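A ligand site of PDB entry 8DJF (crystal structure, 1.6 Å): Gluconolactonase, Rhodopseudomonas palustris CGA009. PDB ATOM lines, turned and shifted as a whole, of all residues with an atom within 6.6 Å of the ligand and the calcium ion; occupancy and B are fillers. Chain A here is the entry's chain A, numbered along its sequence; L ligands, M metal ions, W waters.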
ATOM      1  N   PHE A  16     -34.320  21.264  18.097  1.00  0.00           N
ATOM      2  CA  PHE A  16     -33.201  21.971  18.704  1.00  0.00           C
ATOM      3  C   PHE A  16     -33.717  22.898  19.810  1.00  0.00           C
ATOM      4  O   PHE A  16     -33.763  24.131  19.648  1.00  0.00           O
ATOM      5  CB  PHE A  16     -32.355  22.748  17.687  1.00  0.00           C
ATOM      6  CG  PHE A  16     -30.928  22.933  18.140  1.00  0.00           C
ATOM      7  CD1 PHE A  16     -30.574  23.973  18.979  1.00  0.00           C
ATOM      8  CD2 PHE A  16     -29.947  22.019  17.776  1.00  0.00           C
ATOM      9  CE1 PHE A  16     -29.280  24.112  19.444  1.00  0.00           C
ATOM     10  CE2 PHE A  16     -28.638  22.157  18.225  1.00  0.00           C
ATOM     11  CZ  PHE A  16     -28.297  23.207  19.057  1.00  0.00           C
ATOM     12  N   PRO A  17     -34.106  22.330  20.940  1.00  0.00           N
ATOM     13  CA  PRO A  17     -34.587  23.156  22.047  1.00  0.00           C
ATOM     14  C   PRO A  17     -33.494  24.046  22.632  1.00  0.00           C
ATOM     15  O   PRO A  17     -32.311  23.679  22.669  1.00  0.00           O
ATOM     16  CB  PRO A  17     -35.073  22.127  23.087  1.00  0.00           C
ATOM     17  CG  PRO A  17     -34.253  20.881  22.774  1.00  0.00           C
ATOM     18  CD  PRO A  17     -34.167  20.885  21.252  1.00  0.00           C
ATOM     19  N   GLU A  18     -33.914  25.209  23.119  1.00  0.00           N
ATOM     20  CA  GLU A  18     -33.018  26.171  23.754  1.00  0.00           C
ATOM     21  C   GLU A  18     -33.885  27.147  24.574  1.00  0.00           C
ATOM     22  O   GLU A  18     -35.104  27.044  24.589  1.00  0.00           O
ATOM     23  CB  GLU A  18     -32.147  26.881  22.715  1.00  0.00           C
ATOM     24  CG  GLU A  18     -30.640  26.605  22.807  1.00  0.00           C
ATOM     25  CD  GLU A  18     -29.914  27.587  23.742  1.00  0.00           C
ATOM     26  OE1 GLU A  18     -30.566  28.195  24.601  1.00  0.00           O
ATOM     27  OE2 GLU A  18     -28.667  27.740  23.608  1.00  0.00           O
ATOM     28  N   GLY A  19     -33.208  28.116  25.209  1.00  0.00           N
ATOM     29  CA  GLY A  19     -33.841  29.192  25.956  1.00  0.00           C
ATOM     30  C   GLY A  19     -35.007  28.794  26.822  1.00  0.00           C
ATOM     31  O   GLY A  19     -36.064  29.413  26.735  1.00  0.00           O
ATOM     32  N   ILE A  33     -35.054  26.204  17.872  1.00  0.00           N
ATOM     33  CA  ILE A  33     -34.349  27.016  16.898  1.00  0.00           C
ATOM     34  C   ILE A  33     -34.664  26.523  15.493  1.00  0.00           C
ATOM     35  O   ILE A  33     -34.898  27.318  14.574  1.00  0.00           O
ATOM     36  CB  ILE A  33     -32.826  27.001  17.164  1.00  0.00           C
ATOM     37  CG1 ILE A  33     -32.535  27.195  18.643  1.00  0.00           C
ATOM     38  CG2 ILE A  33     -32.194  28.126  16.368  1.00  0.00           C
ATOM     39  CD1 ILE A  33     -31.063  27.454  18.944  1.00  0.00           C
ATOM     40  N   ASN A  58     -33.233  31.917  19.685  1.00  0.00           N
ATOM     41  CA  ASN A  58     -32.076  31.268  20.324  1.00  0.00           C
ATOM     42  C   ASN A  58     -32.093  31.319  21.852  1.00  0.00           C
ATOM     43  O   ASN A  58     -31.558  30.410  22.502  1.00  0.00           O
ATOM     44  CB  ASN A  58     -30.796  31.968  19.802  1.00  0.00           C
ATOM     45  CG  ASN A  58     -29.533  31.123  19.831  1.00  0.00           C
ATOM     46  OD1 ASN A  58     -28.649  31.327  18.998  1.00  0.00           O
ATOM     47  ND2 ASN A  58     -29.413  30.205  20.797  1.00  0.00           N
ATOM     48  N   GLY A  59     -32.667  32.357  22.446  1.00  0.00           N
ATOM     49  CA  GLY A  59     -32.729  32.471  23.880  1.00  0.00           C
ATOM     50  C   GLY A  59     -33.967  33.280  24.234  1.00  0.00           C
ATOM     51  O   GLY A  59     -34.488  34.028  23.403  1.00  0.00           O
ATOM     52  N   ASN A  73     -31.020  34.815  16.331  1.00  0.00           N
ATOM     53  CA  ASN A  73     -29.705  34.826  15.695  1.00  0.00           C
ATOM     54  C   ASN A  73     -29.788  34.947  14.185  1.00  0.00           C
ATOM     55  O   ASN A  73     -28.743  34.932  13.512  1.00  0.00           O
ATOM     56  CB  ASN A  73     -28.938  33.584  16.114  1.00  0.00           C
ATOM     57  CG  ASN A  73     -29.480  32.296  15.500  1.00  0.00           C
ATOM     58  OD1 ASN A  73     -29.912  32.228  14.343  1.00  0.00           O
ATOM     59  ND2 ASN A  73     -29.401  31.246  16.282  1.00  0.00           N
ATOM     60  N   PHE A  76     -29.737  29.621  11.184  1.00  0.00           N
ATOM     61  CA  PHE A  76     -28.565  28.791  10.928  1.00  0.00           C
ATOM     62  C   PHE A  76     -28.785  27.954   9.663  1.00  0.00           C
ATOM     63  O   PHE A  76     -29.867  27.990   9.049  1.00  0.00           O
ATOM     64  CB  PHE A  76     -28.292  27.847  12.102  1.00  0.00           C
ATOM     65  CG  PHE A  76     -27.686  28.496  13.312  1.00  0.00           C
ATOM     66  CD1 PHE A  76     -26.607  29.359  13.189  1.00  0.00           C
ATOM     67  CD2 PHE A  76     -28.215  28.248  14.582  1.00  0.00           C
ATOM     68  CE1 PHE A  76     -26.041  29.957  14.314  1.00  0.00           C
ATOM     69  CE2 PHE A  76     -27.663  28.847  15.706  1.00  0.00           C
ATOM     70  CZ  PHE A  76     -26.564  29.688  15.572  1.00  0.00           C
ATOM     71  N   TRP A  78     -28.785  23.915   8.736  1.00  0.00           N
ATOM     72  CA  TRP A  78     -28.854  22.638   9.438  1.00  0.00           C
ATOM     73  C   TRP A  78     -28.458  21.441   8.573  1.00  0.00           C
ATOM     74  O   TRP A  78     -28.928  21.294   7.452  1.00  0.00           O
ATOM     75  CB  TRP A  78     -30.284  22.454   9.992  1.00  0.00           C
ATOM     76  CG  TRP A  78     -30.728  23.614  10.882  1.00  0.00           C
ATOM     77  CD1 TRP A  78     -31.362  24.754  10.483  1.00  0.00           C
ATOM     78  CD2 TRP A  78     -30.540  23.720  12.300  1.00  0.00           C
ATOM     79  NE1 TRP A  78     -31.587  25.575  11.581  1.00  0.00           N
ATOM     80  CE2 TRP A  78     -31.089  24.961  12.697  1.00  0.00           C
ATOM     81  CE3 TRP A  78     -29.971  22.887  13.267  1.00  0.00           C
ATOM     82  CZ2 TRP A  78     -31.087  25.384  14.024  1.00  0.00           C
ATOM     83  CZ3 TRP A  78     -29.962  23.314  14.583  1.00  0.00           C
ATOM     84  CH2 TRP A  78     -30.508  24.556  14.946  1.00  0.00           C
ATOM     85  N   PRO A  87     -26.716  22.501  13.837  1.00  0.00           N
ATOM     86  CA  PRO A  87     -26.604  23.783  13.132  1.00  0.00           C
ATOM     87  C   PRO A  87     -25.213  23.971  12.541  1.00  0.00           C
ATOM     88  O   PRO A  87     -24.245  23.299  12.909  1.00  0.00           O
ATOM     89  CB  PRO A  87     -26.907  24.832  14.211  1.00  0.00           C
ATOM     90  CG  PRO A  87     -26.517  24.187  15.491  1.00  0.00           C
ATOM     91  CD  PRO A  87     -26.739  22.681  15.304  1.00  0.00           C
ATOM     92  N   ASN A 126     -27.778  35.679  21.103  1.00  0.00           N
ATOM     93  CA  ASN A 126     -27.804  34.301  21.593  1.00  0.00           C
ATOM     94  C   ASN A 126     -28.603  34.075  22.877  1.00  0.00           C
ATOM     95  O   ASN A 126     -29.559  33.299  22.884  1.00  0.00           O
ATOM     96  CB  ASN A 126     -26.368  33.782  21.779  1.00  0.00           C
ATOM     97  CG  ASN A 126     -26.345  32.289  21.946  1.00  0.00           C
ATOM     98  OD1 ASN A 126     -26.804  31.725  22.961  1.00  0.00           O
ATOM     99  ND2 ASN A 126     -25.858  31.600  20.917  1.00  0.00           N
ATOM    100  N   ASP A 127     -28.221  34.726  23.954  1.00  0.00           N
ATOM    101  CA  ASP A 127     -28.973  34.592  25.204  1.00  0.00           C
ATOM    102  C   ASP A 127     -29.014  35.922  25.942  1.00  0.00           C
ATOM    103  O   ASP A 127     -28.362  36.892  25.568  1.00  0.00           O
ATOM    104  CB  ASP A 127     -28.372  33.499  26.099  1.00  0.00           C
ATOM    105  CG  ASP A 127     -29.460  32.667  26.841  1.00  0.00           C
ATOM    106  OD1 ASP A 127     -30.644  33.169  26.986  1.00  0.00           O
ATOM    107  OD2 ASP A 127     -29.092  31.584  27.343  1.00  0.00           O
ATOM    108  N   THR A 139     -26.008  38.488  24.755  1.00  0.00           N
ATOM    109  CA  THR A 139     -24.796  38.137  24.030  1.00  0.00           C
ATOM    110  C   THR A 139     -25.046  38.071  22.534  1.00  0.00           C
ATOM    111  O   THR A 139     -26.157  37.831  22.080  1.00  0.00           O
ATOM    112  CB  THR A 139     -24.257  36.781  24.505  1.00  0.00           C
ATOM    113  OG1 THR A 139     -25.300  35.838  24.427  1.00  0.00           O
ATOM    114  CG2 THR A 139     -23.623  36.853  25.817  1.00  0.00           C
ATOM    115  N   LEU A 141     -23.218  35.860  19.611  1.00  0.00           N
ATOM    116  CA  LEU A 141     -22.302  34.813  19.199  1.00  0.00           C
ATOM    117  C   LEU A 141     -21.623  35.116  17.878  1.00  0.00           C
ATOM    118  O   LEU A 141     -20.577  34.507  17.564  1.00  0.00           O
ATOM    119  CB  LEU A 141     -23.112  33.510  19.121  1.00  0.00           C
ATOM    120  CG  LEU A 141     -22.295  32.242  18.917  1.00  0.00           C
ATOM    121  CD1 LEU A 141     -21.670  31.801  20.243  1.00  0.00           C
ATOM    122  CD2 LEU A 141     -23.113  31.145  18.315  1.00  0.00           C
ATOM    123  N   ASN A 175     -21.984  33.395  24.480  1.00  0.00           N
ATOM    124  CA  ASN A 175     -23.138  32.525  24.452  1.00  0.00           C
ATOM    125  C   ASN A 175     -23.948  32.731  25.726  1.00  0.00           C
ATOM    126  O   ASN A 175     -24.817  33.606  25.786  1.00  0.00           O
ATOM    127  CB  ASN A 175     -22.658  31.075  24.272  1.00  0.00           C
ATOM    128  CG  ASN A 175     -23.732  30.187  23.712  1.00  0.00           C
ATOM    129  OD1 ASN A 175     -24.857  30.208  24.218  1.00  0.00           O
ATOM    130  ND2 ASN A 175     -23.428  29.428  22.668  1.00  0.00           N
ATOM    131  N   GLY A 176     -23.701  31.952  26.762  1.00  0.00           N
ATOM    132  CA  GLY A 176     -24.452  32.146  27.994  1.00  0.00           C
ATOM    133  C   GLY A 176     -24.150  33.478  28.625  1.00  0.00           C
ATOM    134  O   GLY A 176     -23.071  34.051  28.468  1.00  0.00           O
ATOM    135  N   THR A 191     -17.745  30.450  23.887  1.00  0.00           N
ATOM    136  CA  THR A 191     -18.070  29.095  23.451  1.00  0.00           C
ATOM    137  C   THR A 191     -16.859  28.235  23.105  1.00  0.00           C
ATOM    138  O   THR A 191     -16.681  27.173  23.708  1.00  0.00           O
ATOM    139  CB  THR A 191     -19.029  29.163  22.262  1.00  0.00           C
ATOM    140  OG1 THR A 191     -20.307  29.603  22.728  1.00  0.00           O
ATOM    141  CG2 THR A 191     -19.218  27.829  21.634  1.00  0.00           C
ATOM    142  N   PHE A 231     -18.526  25.822  25.705  1.00  0.00           N
ATOM    143  CA  PHE A 231     -19.612  26.327  26.540  1.00  0.00           C
ATOM    144  C   PHE A 231     -20.774  26.814  25.696  1.00  0.00           C
ATOM    145  O   PHE A 231     -20.586  27.446  24.656  1.00  0.00           O
ATOM    146  CB  PHE A 231     -19.144  27.492  27.424  1.00  0.00           C
ATOM    147  CG  PHE A 231     -18.454  27.089  28.691  1.00  0.00           C
ATOM    148  CD1 PHE A 231     -18.762  25.886  29.331  1.00  0.00           C
ATOM    149  CD2 PHE A 231     -17.585  27.976  29.317  1.00  0.00           C
ATOM    150  CE1 PHE A 231     -18.145  25.548  30.501  1.00  0.00           C
ATOM    151  CE2 PHE A 231     -17.004  27.661  30.514  1.00  0.00           C
ATOM    152  CZ  PHE A 231     -17.280  26.457  31.121  1.00  0.00           C
ATOM    153  N   ASP A 232     -21.990  26.621  26.226  1.00  0.00           N
ATOM    154  CA  ASP A 232     -23.208  27.164  25.616  1.00  0.00           C
ATOM    155  C   ASP A 232     -23.814  28.116  26.635  1.00  0.00           C
ATOM    156  O   ASP A 232     -23.146  29.054  27.061  1.00  0.00           O
ATOM    157  CB  ASP A 232     -24.126  26.038  25.185  1.00  0.00           C
ATOM    158  CG  ASP A 232     -25.083  26.452  24.077  1.00  0.00           C
ATOM    159  OD1 ASP A 232     -25.716  27.548  24.187  1.00  0.00           O
ATOM    160  OD2 ASP A 232     -25.234  25.676  23.114  1.00  0.00           O
ATOM    161  N   SER A 233     -25.074  27.931  27.005  1.00  0.00           N
ATOM    162  CA  SER A 233     -25.800  28.864  27.881  1.00  0.00           C
ATOM    163  C   SER A 233     -25.634  28.500  29.352  1.00  0.00           C
ATOM    164  O   SER A 233     -25.102  27.459  29.699  1.00  0.00           O
ATOM    165  CB  SER A 233     -27.266  28.911  27.458  1.00  0.00           C
ATOM    166  OG  SER A 233     -27.402  29.741  26.321  1.00  0.00           O
ATOM    167  N   LEU A 234     -26.198  29.337  30.245  1.00  0.00           N
ATOM    168  CA  LEU A 234     -25.911  29.185  31.660  1.00  0.00           C
ATOM    169  C   LEU A 234     -27.079  29.669  32.518  1.00  0.00           C
ATOM    170  O   LEU A 234     -28.027  30.301  32.022  1.00  0.00           O
ATOM    171  CB  LEU A 234     -24.630  29.941  32.048  1.00  0.00           C
ATOM    172  CG  LEU A 234     -24.604  31.450  31.914  1.00  0.00           C
ATOM    173  CD1 LEU A 234     -25.287  32.151  33.102  1.00  0.00           C
ATOM    174  CD2 LEU A 234     -23.212  31.998  31.728  1.00  0.00           C
ATOM    175  N   LEU A 247     -20.745  21.672  26.072  1.00  0.00           N
ATOM    176  CA  LEU A 247     -20.793  20.901  24.868  1.00  0.00           C
ATOM    177  C   LEU A 247     -19.561  19.985  24.766  1.00  0.00           C
ATOM    178  O   LEU A 247     -18.534  20.236  25.398  1.00  0.00           O
ATOM    179  CB  LEU A 247     -20.845  21.823  23.670  1.00  0.00           C
ATOM    180  CG  LEU A 247     -21.955  22.856  23.609  1.00  0.00           C
ATOM    181  CD1 LEU A 247     -21.525  23.946  22.630  1.00  0.00           C
ATOM    182  CD2 LEU A 247     -23.211  22.190  23.178  1.00  0.00           C
ATOM    183  N   VAL A 271     -24.539  17.604  23.026  1.00  0.00           N
ATOM    184  CA  VAL A 271     -25.069  18.919  22.673  1.00  0.00           C
ATOM    185  C   VAL A 271     -26.040  19.406  23.754  1.00  0.00           C
ATOM    186  O   VAL A 271     -27.224  19.635  23.477  1.00  0.00           O
ATOM    187  CB  VAL A 271     -25.776  18.868  21.304  1.00  0.00           C
ATOM    188  CG1 VAL A 271     -26.081  20.262  20.790  1.00  0.00           C
ATOM    189  CG2 VAL A 271     -24.903  18.126  20.292  1.00  0.00           C
ATOM    190  N   THR A 273     -27.264  22.394  25.955  1.00  0.00           N
ATOM    191  CA  THR A 273     -27.170  23.774  25.517  1.00  0.00           C
ATOM    192  C   THR A 273     -27.602  24.793  26.561  1.00  0.00           C
ATOM    193  O   THR A 273     -27.106  25.916  26.543  1.00  0.00           O
ATOM    194  CB  THR A 273     -28.032  24.003  24.262  1.00  0.00           C
ATOM    195  OG1 THR A 273     -29.378  23.557  24.517  1.00  0.00           O
ATOM    196  CG2 THR A 273     -27.475  23.243  23.069  1.00  0.00           C
ATOM    197  N   ASN A 274     -28.517  24.451  27.470  1.00  0.00           N
ATOM    198  CA  ASN A 274     -29.003  25.474  28.384  1.00  0.00           C
ATOM    199  C   ASN A 274     -29.566  24.803  29.632  1.00  0.00           C
ATOM    200  O   ASN A 274     -29.862  23.602  29.647  1.00  0.00           O
ATOM    201  CB  ASN A 274     -30.046  26.410  27.707  1.00  0.00           C
ATOM    202  CG  ASN A 274     -30.019  27.854  28.232  1.00  0.00           C
ATOM    203  OD1 ASN A 274     -29.684  28.126  29.403  1.00  0.00           O
ATOM    204  ND2 ASN A 274     -30.321  28.789  27.345  1.00  0.00           N
ATOM    205  N   SER A 290     -30.147  19.391  23.176  1.00  0.00           N
ATOM    206  CA  SER A 290     -30.512  19.774  21.817  1.00  0.00           C
ATOM    207  C   SER A 290     -30.088  18.751  20.783  1.00  0.00           C
ATOM    208  O   SER A 290     -30.568  18.810  19.642  1.00  0.00           O
ATOM    209  CB  SER A 290     -29.923  21.130  21.498  1.00  0.00           C
ATOM    210  OG  SER A 290     -30.437  22.123  22.379  1.00  0.00           O
HETATM  211  C1  LIG L   1     -26.614  27.525  20.737  1.00  0.00           C
HETATM  212  C2  LIG L   1     -27.300  27.733  19.397  1.00  0.00           C
HETATM  213  C3  LIG L   1     -26.133  27.982  18.436  1.00  0.00           C
HETATM  214  C4  LIG L   1     -24.924  27.311  19.107  1.00  0.00           C
HETATM  215  C5  LIG L   1     -24.431  26.031  18.462  1.00  0.00           C
HETATM  216  O1  LIG L   1     -27.275  26.566  21.538  1.00  0.00           O
HETATM  217  O2  LIG L   1     -26.516  28.723  21.379  1.00  0.00           O
HETATM  218  O3  LIG L   1     -25.310  27.061  20.474  1.00  0.00           O
HETATM  219 CA    CA M   1     -27.051  29.532  23.854  1.00  0.00          CA
HETATM  220  O   HOH W   1     -29.056  30.606  24.213  1.00  0.00           O
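The calcium ion is bound by water W1 (2.3 Å), the side-chain amide oxygen of Asn 175 (2.3 Å), the side-chain amide oxygen of Asn 126 (2.4 Å), the side-chain carboxylate of Asp 232 (2.4 Å), the side-chain carboxylate of Glu 18 (2.4 Å), the side-chain hydroxyl of Ser 233 (2.5 Å) and an oxygen (O2) of the ligand (2.7 Å).
The side-chain hydroxyl (OG1) of Thr 191 sits at hydrogen-bond distance from the side-chain amide nitrogen (ND2) of Asn 175, 3.1 Å away. O of Asn 126 lies within hydrogen-bond range of N of Gly 59, at 3.3 Å. OE1 of Glu 18 sits at hydrogen-bond distance from ND2 of Asn 274, 2.8 Å away. O of Thr 273 is in hydrogen-bond range of N of Ser 233 (2.9 Å). OG of Ser 233 sits close to OD2 of Asp 127, at 2.7 Å. The side-chain hydroxyl (OG) of Ser 233 lies close to the side-chain amide nitrogen (ND2) of Asn 274, 3.2 Å away. The side-chain hydroxyl (OG1) of Thr 273 is in hydrogen-bond range of the side-chain hydroxyl (OG) of Ser 290 (2.8 Å). The side-chain hydroxyl of Thr 273 sits at hydrogen-bond distance from the backbone carbonyl oxygen of Pro 17 (3.5 Å).
Merely in contact with the ligand: Phe 76, Thr 273, Phe 16 and Ile 33. Within 4 Å of the ligand: Phe 16, Glu 18, Ile 33, Asn 58, Phe 76, Asn 126, Asn 175, Asp 232 and Thr 273. The nearest printed residue that does not touch the ligand is Pro 87 (4.1 Å).
Residues that only touch the calcium ion: Asn 58 (3.9 Å). Along chain A the residues within 4 Å of the calcium ion span positions 18 to 233.
The side-chain amide nitrogen (ND2) of Asn 58 lies close to an oxygen (O2) of the ligand.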
